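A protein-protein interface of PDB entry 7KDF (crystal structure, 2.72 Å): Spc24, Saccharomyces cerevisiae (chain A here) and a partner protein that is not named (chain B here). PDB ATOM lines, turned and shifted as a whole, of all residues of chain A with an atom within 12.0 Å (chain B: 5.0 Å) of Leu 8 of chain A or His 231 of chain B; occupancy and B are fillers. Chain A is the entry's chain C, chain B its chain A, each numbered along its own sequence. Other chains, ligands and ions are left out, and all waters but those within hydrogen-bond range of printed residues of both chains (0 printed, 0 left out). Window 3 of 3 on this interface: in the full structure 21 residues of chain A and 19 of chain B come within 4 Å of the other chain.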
ATOM      1  N   ASP A   5      27.597   4.647  -0.251  1.00  0.00           N
ATOM      2  CA  ASP A   5      28.238   5.257   0.907  1.00  0.00           C
ATOM      3  C   ASP A   5      27.303   6.235   1.606  1.00  0.00           C
ATOM      4  O   ASP A   5      27.607   6.717   2.699  1.00  0.00           O
ATOM      5  CB  ASP A   5      29.524   5.975   0.495  1.00  0.00           C
ATOM      6  CG  ASP A   5      30.765   5.142   0.746  1.00  0.00           C
ATOM      7  OD1 ASP A   5      30.635   4.030   1.297  1.00  0.00           O
ATOM      8  OD2 ASP A   5      31.872   5.603   0.395  1.00  0.00           O
ATOM      9  N   ASN A   6      26.170   6.526   0.963  1.00  0.00           N
ATOM     10  CA  ASN A   6      25.227   7.558   1.398  1.00  0.00           C
ATOM     11  C   ASN A   6      25.891   8.926   1.507  1.00  0.00           C
ATOM     12  O   ASN A   6      25.379   9.824   2.184  1.00  0.00           O
ATOM     13  CB  ASN A   6      24.552   7.184   2.723  1.00  0.00           C
ATOM     14  CG  ASN A   6      23.793   5.875   2.637  1.00  0.00           C
ATOM     15  OD1 ASN A   6      24.383   4.813   2.439  1.00  0.00           O
ATOM     16  ND2 ASN A   6      22.475   5.946   2.780  1.00  0.00           N
ATOM     17  N   LEU A   7      27.029   9.088   0.847  1.00  0.00           N
ATOM     18  CA  LEU A   7      27.781  10.324   0.807  1.00  0.00           C
ATOM     19  C   LEU A   7      27.723  10.904  -0.600  1.00  0.00           C
ATOM     20  O   LEU A   7      26.982  10.426  -1.469  1.00  0.00           O
ATOM     21  CB  LEU A   7      29.224  10.083   1.251  1.00  0.00           C
ATOM     22  CG  LEU A   7      29.463   9.899   2.748  1.00  0.00           C
ATOM     23  CD1 LEU A   7      30.946  10.020   3.068  1.00  0.00           C
ATOM     24  CD2 LEU A   7      28.651  10.901   3.555  1.00  0.00           C
ATOM     25  N   LEU A   8      28.503  11.950  -0.827  1.00  0.00           N
ATOM     26  CA  LEU A   8      28.632  12.549  -2.140  1.00  0.00           C
ATOM     27  C   LEU A   8      30.013  12.261  -2.701  1.00  0.00           C
ATOM     28  O   LEU A   8      31.032  12.587  -2.085  1.00  0.00           O
ATOM     29  CB  LEU A   8      28.374  14.055  -2.088  1.00  0.00           C
ATOM     30  CG  LEU A   8      26.893  14.423  -1.902  1.00  0.00           C
ATOM     31  CD1 LEU A   8      26.646  15.874  -2.260  1.00  0.00           C
ATOM     32  CD2 LEU A   8      25.989  13.510  -2.737  1.00  0.00           C
ATOM     33  N   ASP A   9      30.020  11.671  -3.887  1.00  0.00           N
ATOM     34  CA  ASP A   9      31.232  11.482  -4.671  1.00  0.00           C
ATOM     35  C   ASP A   9      32.057  12.745  -4.788  1.00  0.00           C
ATOM     36  O   ASP A   9      33.263  12.749  -4.545  1.00  0.00           O
ATOM     37  CB  ASP A   9      30.794  10.960  -6.027  1.00  0.00           C
ATOM     38  CG  ASP A   9      30.426   9.500  -5.963  1.00  0.00           C
ATOM     39  OD1 ASP A   9      31.198   8.792  -5.283  1.00  0.00           O
ATOM     40  OD2 ASP A   9      29.317   9.101  -6.418  1.00  0.00           O
ATOM     41  N   ASN A  10      31.408  13.881  -5.130  1.00  0.00           N
ATOM     42  CA  ASN A  10      32.100  15.156  -5.168  1.00  0.00           C
ATOM     43  C   ASN A  10      31.090  16.278  -4.871  1.00  0.00           C
ATOM     44  O   ASN A  10      30.477  16.822  -5.782  1.00  0.00           O
ATOM     45  CB  ASN A  10      32.800  15.418  -6.506  1.00  0.00           C
ATOM     46  CG  ASN A  10      33.904  16.459  -6.402  1.00  0.00           C
ATOM     47  OD1 ASN A  10      33.974  17.222  -5.438  1.00  0.00           O
ATOM     48  ND2 ASN A  10      34.768  16.503  -7.417  1.00  0.00           N
ATOM     49  N   PRO A  11      30.932  16.604  -3.590  1.00  0.00           N
ATOM     50  CA  PRO A  11      29.980  17.689  -3.256  1.00  0.00           C
ATOM     51  C   PRO A  11      30.389  19.050  -3.783  1.00  0.00           C
ATOM     52  O   PRO A  11      29.514  19.900  -3.987  1.00  0.00           O
ATOM     53  CB  PRO A  11      29.960  17.663  -1.720  1.00  0.00           C
ATOM     54  CG  PRO A  11      31.249  17.046  -1.326  1.00  0.00           C
ATOM     55  CD  PRO A  11      31.582  16.053  -2.403  1.00  0.00           C
ATOM     56  N   VAL A  12      31.682  19.289  -4.008  1.00  0.00           N
ATOM     57  CA  VAL A  12      32.119  20.587  -4.513  1.00  0.00           C
ATOM     58  C   VAL A  12      31.664  20.781  -5.953  1.00  0.00           C
ATOM     59  O   VAL A  12      31.099  21.821  -6.308  1.00  0.00           O
ATOM     60  CB  VAL A  12      33.645  20.726  -4.385  1.00  0.00           C
ATOM     61  CG1 VAL A  12      34.107  22.044  -4.996  1.00  0.00           C
ATOM     62  CG2 VAL A  12      34.071  20.622  -2.930  1.00  0.00           C
ATOM     63  N   GLU A  13      31.907  19.785  -6.809  1.00  0.00           N
ATOM     64  CA  GLU A  13      31.393  19.861  -8.169  1.00  0.00           C
ATOM     65  C   GLU A  13      29.880  19.840  -8.178  1.00  0.00           C
ATOM     66  O   GLU A  13      29.260  20.491  -9.024  1.00  0.00           O
ATOM     67  CB  GLU A  13      31.947  18.729  -9.041  1.00  0.00           C
ATOM     68  CG  GLU A  13      33.438  18.813  -9.260  1.00  0.00           C
ATOM     69  CD  GLU A  13      33.827  19.909 -10.250  1.00  0.00           C
ATOM     70  OE1 GLU A  13      33.297  19.921 -11.383  1.00  0.00           O
ATOM     71  OE2 GLU A  13      34.641  20.781  -9.877  1.00  0.00           O
ATOM     72  N   PHE A  14      29.262  19.090  -7.261  1.00  0.00           N
ATOM     73  CA  PHE A  14      27.813  18.966  -7.323  1.00  0.00           C
ATOM     74  C   PHE A  14      27.213  20.366  -7.254  1.00  0.00           C
ATOM     75  O   PHE A  14      26.432  20.778  -8.119  1.00  0.00           O
ATOM     76  CB  PHE A  14      27.254  18.187  -6.139  1.00  0.00           C
ATOM     77  CG  PHE A  14      25.981  17.447  -6.448  1.00  0.00           C
ATOM     78  CD1 PHE A  14      26.015  16.079  -6.558  1.00  0.00           C
ATOM     79  CD2 PHE A  14      24.893  18.102  -7.011  1.00  0.00           C
ATOM     80  CE1 PHE A  14      24.888  15.362  -6.883  1.00  0.00           C
ATOM     81  CE2 PHE A  14      23.760  17.400  -7.388  1.00  0.00           C
ATOM     82  CZ  PHE A  14      23.767  16.024  -7.330  1.00  0.00           C
ATOM     83  N   LEU A  15      27.632  21.127  -6.231  1.00  0.00           N
ATOM     84  CA  LEU A  15      27.166  22.495  -6.016  1.00  0.00           C
ATOM     85  C   LEU A  15      27.547  23.402  -7.173  1.00  0.00           C
ATOM     86  O   LEU A  15      26.752  24.246  -7.605  1.00  0.00           O
ATOM     87  CB  LEU A  15      27.762  23.054  -4.723  1.00  0.00           C
ATOM     88  CG  LEU A  15      27.227  22.609  -3.366  1.00  0.00           C
ATOM     89  CD1 LEU A  15      28.137  23.112  -2.257  1.00  0.00           C
ATOM     90  CD2 LEU A  15      25.827  23.154  -3.179  1.00  0.00           C
ATOM     91  N   LYS A  16      28.777  23.264  -7.662  1.00  0.00           N
ATOM     92  CA  LYS A  16      29.243  24.076  -8.778  1.00  0.00           C
ATOM     93  C   LYS A  16      28.340  23.902  -9.999  1.00  0.00           C
ATOM     94  O   LYS A  16      27.917  24.885 -10.620  1.00  0.00           O
ATOM     95  CB  LYS A  16      30.682  23.693  -9.104  1.00  0.00           C
ATOM     96  CG  LYS A  16      31.289  24.497 -10.224  1.00  0.00           C
ATOM     97  CD  LYS A  16      32.685  23.987 -10.514  1.00  0.00           C
ATOM     98  CE  LYS A  16      33.291  24.693 -11.719  1.00  0.00           C
ATOM     99  NZ  LYS A  16      34.670  24.179 -11.911  1.00  0.00           N
ATOM    100  N   GLU A  17      27.998  22.651 -10.327  1.00  0.00           N
ATOM    101  CA  GLU A  17      27.114  22.381 -11.461  1.00  0.00           C
ATOM    102  C   GLU A  17      25.766  23.081 -11.314  1.00  0.00           C
ATOM    103  O   GLU A  17      25.213  23.595 -12.297  1.00  0.00           O
ATOM    104  CB  GLU A  17      26.913  20.874 -11.616  1.00  0.00           C
ATOM    105  CG  GLU A  17      28.199  20.116 -11.882  1.00  0.00           C
ATOM    106  CD  GLU A  17      28.006  18.621 -11.844  1.00  0.00           C
ATOM    107  OE1 GLU A  17      29.016  17.885 -11.889  1.00  0.00           O
ATOM    108  OE2 GLU A  17      26.837  18.185 -11.772  1.00  0.00           O
ATOM    109  N   VAL A  18      25.214  23.102 -10.100  1.00  0.00           N
ATOM    110  CA  VAL A  18      23.915  23.735  -9.897  1.00  0.00           C
ATOM    111  C   VAL A  18      24.019  25.232 -10.161  1.00  0.00           C
ATOM    112  O   VAL A  18      23.147  25.832 -10.800  1.00  0.00           O
ATOM    113  CB  VAL A  18      23.403  23.448  -8.476  1.00  0.00           C
ATOM    114  CG1 VAL A  18      22.018  24.044  -8.286  1.00  0.00           C
ATOM    115  CG2 VAL A  18      23.444  21.971  -8.184  1.00  0.00           C
ATOM    116  N   ARG B 227      30.730  14.641   8.757  1.00  0.00           N
ATOM    117  CA  ARG B 227      30.765  14.675   7.298  1.00  0.00           C
ATOM    118  C   ARG B 227      29.425  14.269   6.703  1.00  0.00           C
ATOM    119  O   ARG B 227      28.944  14.897   5.754  1.00  0.00           O
ATOM    120  CB  ARG B 227      31.873  13.764   6.776  1.00  0.00           C
ATOM    121  CG  ARG B 227      31.779  13.484   5.290  1.00  0.00           C
ATOM    122  CD  ARG B 227      32.912  12.595   4.820  1.00  0.00           C
ATOM    123  NE  ARG B 227      34.212  13.148   5.178  1.00  0.00           N
ATOM    124  CZ  ARG B 227      35.047  12.581   6.043  1.00  0.00           C
ATOM    125  NH1 ARG B 227      34.713  11.441   6.639  1.00  0.00           N
ATOM    126  NH2 ARG B 227      36.212  13.154   6.310  1.00  0.00           N
ATOM    127  N   TYR B 228      28.809  13.218   7.246  1.00  0.00           N
ATOM    128  CA  TYR B 228      27.501  12.805   6.754  1.00  0.00           C
ATOM    129  C   TYR B 228      26.482  13.923   6.922  1.00  0.00           C
ATOM    130  O   TYR B 228      25.698  14.200   6.006  1.00  0.00           O
ATOM    131  CB  TYR B 228      27.039  11.535   7.477  1.00  0.00           C
ATOM    132  CG  TYR B 228      25.646  11.084   7.089  1.00  0.00           C
ATOM    133  CD1 TYR B 228      25.449  10.209   6.025  1.00  0.00           C
ATOM    134  CD2 TYR B 228      24.530  11.530   7.788  1.00  0.00           C
ATOM    135  CE1 TYR B 228      24.176   9.796   5.665  1.00  0.00           C
ATOM    136  CE2 TYR B 228      23.257  11.125   7.436  1.00  0.00           C
ATOM    137  CZ  TYR B 228      23.083  10.258   6.377  1.00  0.00           C
ATOM    138  OH  TYR B 228      21.812   9.856   6.033  1.00  0.00           O
ATOM    139  N   LYS B 229      26.486  14.585   8.081  1.00  0.00           N
ATOM    140  CA  LYS B 229      25.555  15.687   8.299  1.00  0.00           C
ATOM    141  C   LYS B 229      25.804  16.811   7.305  1.00  0.00           C
ATOM    142  O   LYS B 229      24.856  17.391   6.762  1.00  0.00           O
ATOM    143  CB  LYS B 229      25.675  16.198   9.736  1.00  0.00           C
ATOM    144  CG  LYS B 229      24.655  15.580  10.684  1.00  0.00           C
ATOM    145  CD  LYS B 229      24.427  16.439  11.918  1.00  0.00           C
ATOM    146  CE  LYS B 229      23.512  15.730  12.910  1.00  0.00           C
ATOM    147  NZ  LYS B 229      22.136  15.536  12.368  1.00  0.00           N
ATOM    148  N   LEU B 230      27.076  17.124   7.048  1.00  0.00           N
ATOM    149  CA  LEU B 230      27.411  18.180   6.099  1.00  0.00           C
ATOM    150  C   LEU B 230      26.938  17.833   4.693  1.00  0.00           C
ATOM    151  O   LEU B 230      26.398  18.689   3.985  1.00  0.00           O
ATOM    152  CB  LEU B 230      28.919  18.430   6.110  1.00  0.00           C
ATOM    153  CG  LEU B 230      29.444  19.562   5.231  1.00  0.00           C
ATOM    154  CD1 LEU B 230      28.775  20.874   5.606  1.00  0.00           C
ATOM    155  CD2 LEU B 230      30.955  19.665   5.361  1.00  0.00           C
ATOM    156  N   HIS B 231      27.135  16.582   4.269  1.00  0.00           N
ATOM    157  CA  HIS B 231      26.676  16.181   2.944  1.00  0.00           C
ATOM    158  C   HIS B 231      25.161  16.301   2.824  1.00  0.00           C
ATOM    159  O   HIS B 231      24.653  16.792   1.811  1.00  0.00           O
ATOM    160  CB  HIS B 231      27.134  14.757   2.633  1.00  0.00           C
ATOM    161  CG  HIS B 231      28.566  14.665   2.210  1.00  0.00           C
ATOM    162  ND1 HIS B 231      29.044  13.648   1.415  1.00  0.00           N
ATOM    163  CD2 HIS B 231      29.627  15.466   2.474  1.00  0.00           C
ATOM    164  CE1 HIS B 231      30.337  13.824   1.205  1.00  0.00           C
ATOM    165  NE2 HIS B 231      30.717  14.919   1.840  1.00  0.00           N
ATOM    166  N   GLN B 232      24.425  15.873   3.853  1.00  0.00           N
ATOM    167  CA  GLN B 232      22.976  16.055   3.854  1.00  0.00           C
ATOM    168  C   GLN B 232      22.609  17.527   3.722  1.00  0.00           C
ATOM    169  O   GLN B 232      21.631  17.875   3.049  1.00  0.00           O
ATOM    170  CB  GLN B 232      22.372  15.473   5.131  1.00  0.00           C
ATOM    171  CG  GLN B 232      22.567  13.978   5.286  1.00  0.00           C
ATOM    172  CD  GLN B 232      21.872  13.188   4.202  1.00  0.00           C
ATOM    173  OE1 GLN B 232      20.644  13.096   4.179  1.00  0.00           O
ATOM    174  NE2 GLN B 232      22.652  12.607   3.298  1.00  0.00           N
ATOM    175  N   GLN B 233      23.381  18.407   4.364  1.00  0.00           N
ATOM    176  CA  GLN B 233      23.161  19.840   4.207  1.00  0.00           C
ATOM    177  C   GLN B 233      23.341  20.258   2.753  1.00  0.00           C
ATOM    178  O   GLN B 233      22.539  21.032   2.213  1.00  0.00           O
ATOM    179  CB  GLN B 233      24.130  20.612   5.098  1.00  0.00           C
ATOM    180  CG  GLN B 233      23.595  20.998   6.463  1.00  0.00           C
ATOM    181  CD  GLN B 233      24.624  21.780   7.263  1.00  0.00           C
ATOM    182  OE1 GLN B 233      25.651  21.237   7.672  1.00  0.00           O
ATOM    183  NE2 GLN B 233      24.352  23.061   7.490  1.00  0.00           N
ATOM    184  N   VAL B 234      24.387  19.742   2.102  1.00  0.00           N
ATOM    185  CA  VAL B 234      24.607  20.027   0.687  1.00  0.00           C
ATOM    186  C   VAL B 234      23.449  19.495  -0.148  1.00  0.00           C
ATOM    187  O   VAL B 234      22.982  20.160  -1.079  1.00  0.00           O
ATOM    188  CB  VAL B 234      25.955  19.442   0.224  1.00  0.00           C
ATOM    189  CG1 VAL B 234      26.095  19.546  -1.287  1.00  0.00           C
ATOM    190  CG2 VAL B 234      27.100  20.154   0.914  1.00  0.00           C
ATOM    191  N   ILE B 235      22.958  18.297   0.177  1.00  0.00           N
ATOM    192  CA  ILE B 235      21.829  17.736  -0.562  1.00  0.00           C
ATOM    193  C   ILE B 235      20.637  18.678  -0.482  1.00  0.00           C
ATOM    194  O   ILE B 235      19.975  18.962  -1.488  1.00  0.00           O
ATOM    195  CB  ILE B 235      21.452  16.351  -0.010  1.00  0.00           C
ATOM    196  CG1 ILE B 235      22.648  15.403  -0.025  1.00  0.00           C
ATOM    197  CG2 ILE B 235      20.357  15.733  -0.876  1.00  0.00           C
ATOM    198  CD1 ILE B 235      23.201  15.154  -1.368  1.00  0.00           C
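N of Leu 8 of chain A sits at hydrogen-bond distance from ND1 of His 231 of chain B.
Asn 6 of chain A touches Tyr 228 of chain B.
Leu 7 of chain A touches Arg 227 of chain B.
Tyr 228 of chain B touches Leu 7 of chain A (CA to CD2, 3.9 Å).
CD2 of Leu 7 of chain A touches ND1 of His 231 of chain B, 3.5 Å away.
CD1 of Leu 8 of chain A touches CG1 of Val 234 of chain B, at 3.8 Å.
CD1 of Ile 235 of chain B touches CD2 of Leu 8 of chain A, 3.5 Å away.
NE2 of His 231 of chain B touches CG of Pro 11 of chain A (3.9 Å).
Leu 15 of chain A touches Val 234 of chain B.
Of the printed residues of chain B, Asn 6 of chain A touches Tyr 228.
Of the printed residues of chain B, Leu 7 of chain A touches Arg 227 (3.7 Å), Tyr 228 (3.9 Å) and His 231 (3.5 Å).
Printed residues of chain B within 4 Å of Leu 8 of chain A: His 231 (2.9 Å), Val 234 (3.8 Å) and Ile 235 (3.5 Å).
Of the printed residues of chain B, Pro 11 of chain A touches His 231.
Of the printed residues of chain B, Leu 15 of chain A touches Val 234.
Of chain A, only Leu 7 comes within 4 Å of Arg 227 of chain B.
Of chain A, only Asn 6 and Leu 7 come within 4 Å of Tyr 228 of chain B.
No residue of chain A comes within 4 Å of Leu 230 of chain B.
Of the printed residues of chain A, His 231 of chain B touches Leu 7, Leu 8 and Pro 11.
No residue of chain A comes within 4 Å of Gln 232 of chain B.
No residue of chain A comes within 4 Å of Gln 233 of chain B.
Val 234 of chain B touches two residues of chain A.
Of chain A, only Leu 8 comes within 4 Å of Ile 235 of chain B.
The nearest printed residue of chain B that does not touch Leu 8 of chain A is Gln 232 of chain B (6.4 Å).
Along chain B the printed residues that touch a printed residue of chain A span positions 227 to 235.
Of the 14 printed residues of chain A, 5 touch a printed residue of chain B.
Hydrophobic or aromatic side chains of chain A that line the printed part of chain B: Leu 7, Leu 8, Pro 11 and Leu 15.
Among the printed residues, no Asp or Glu carboxylate lies within 4 Å of a Lys or Arg side-chain nitrogen of the other chain.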
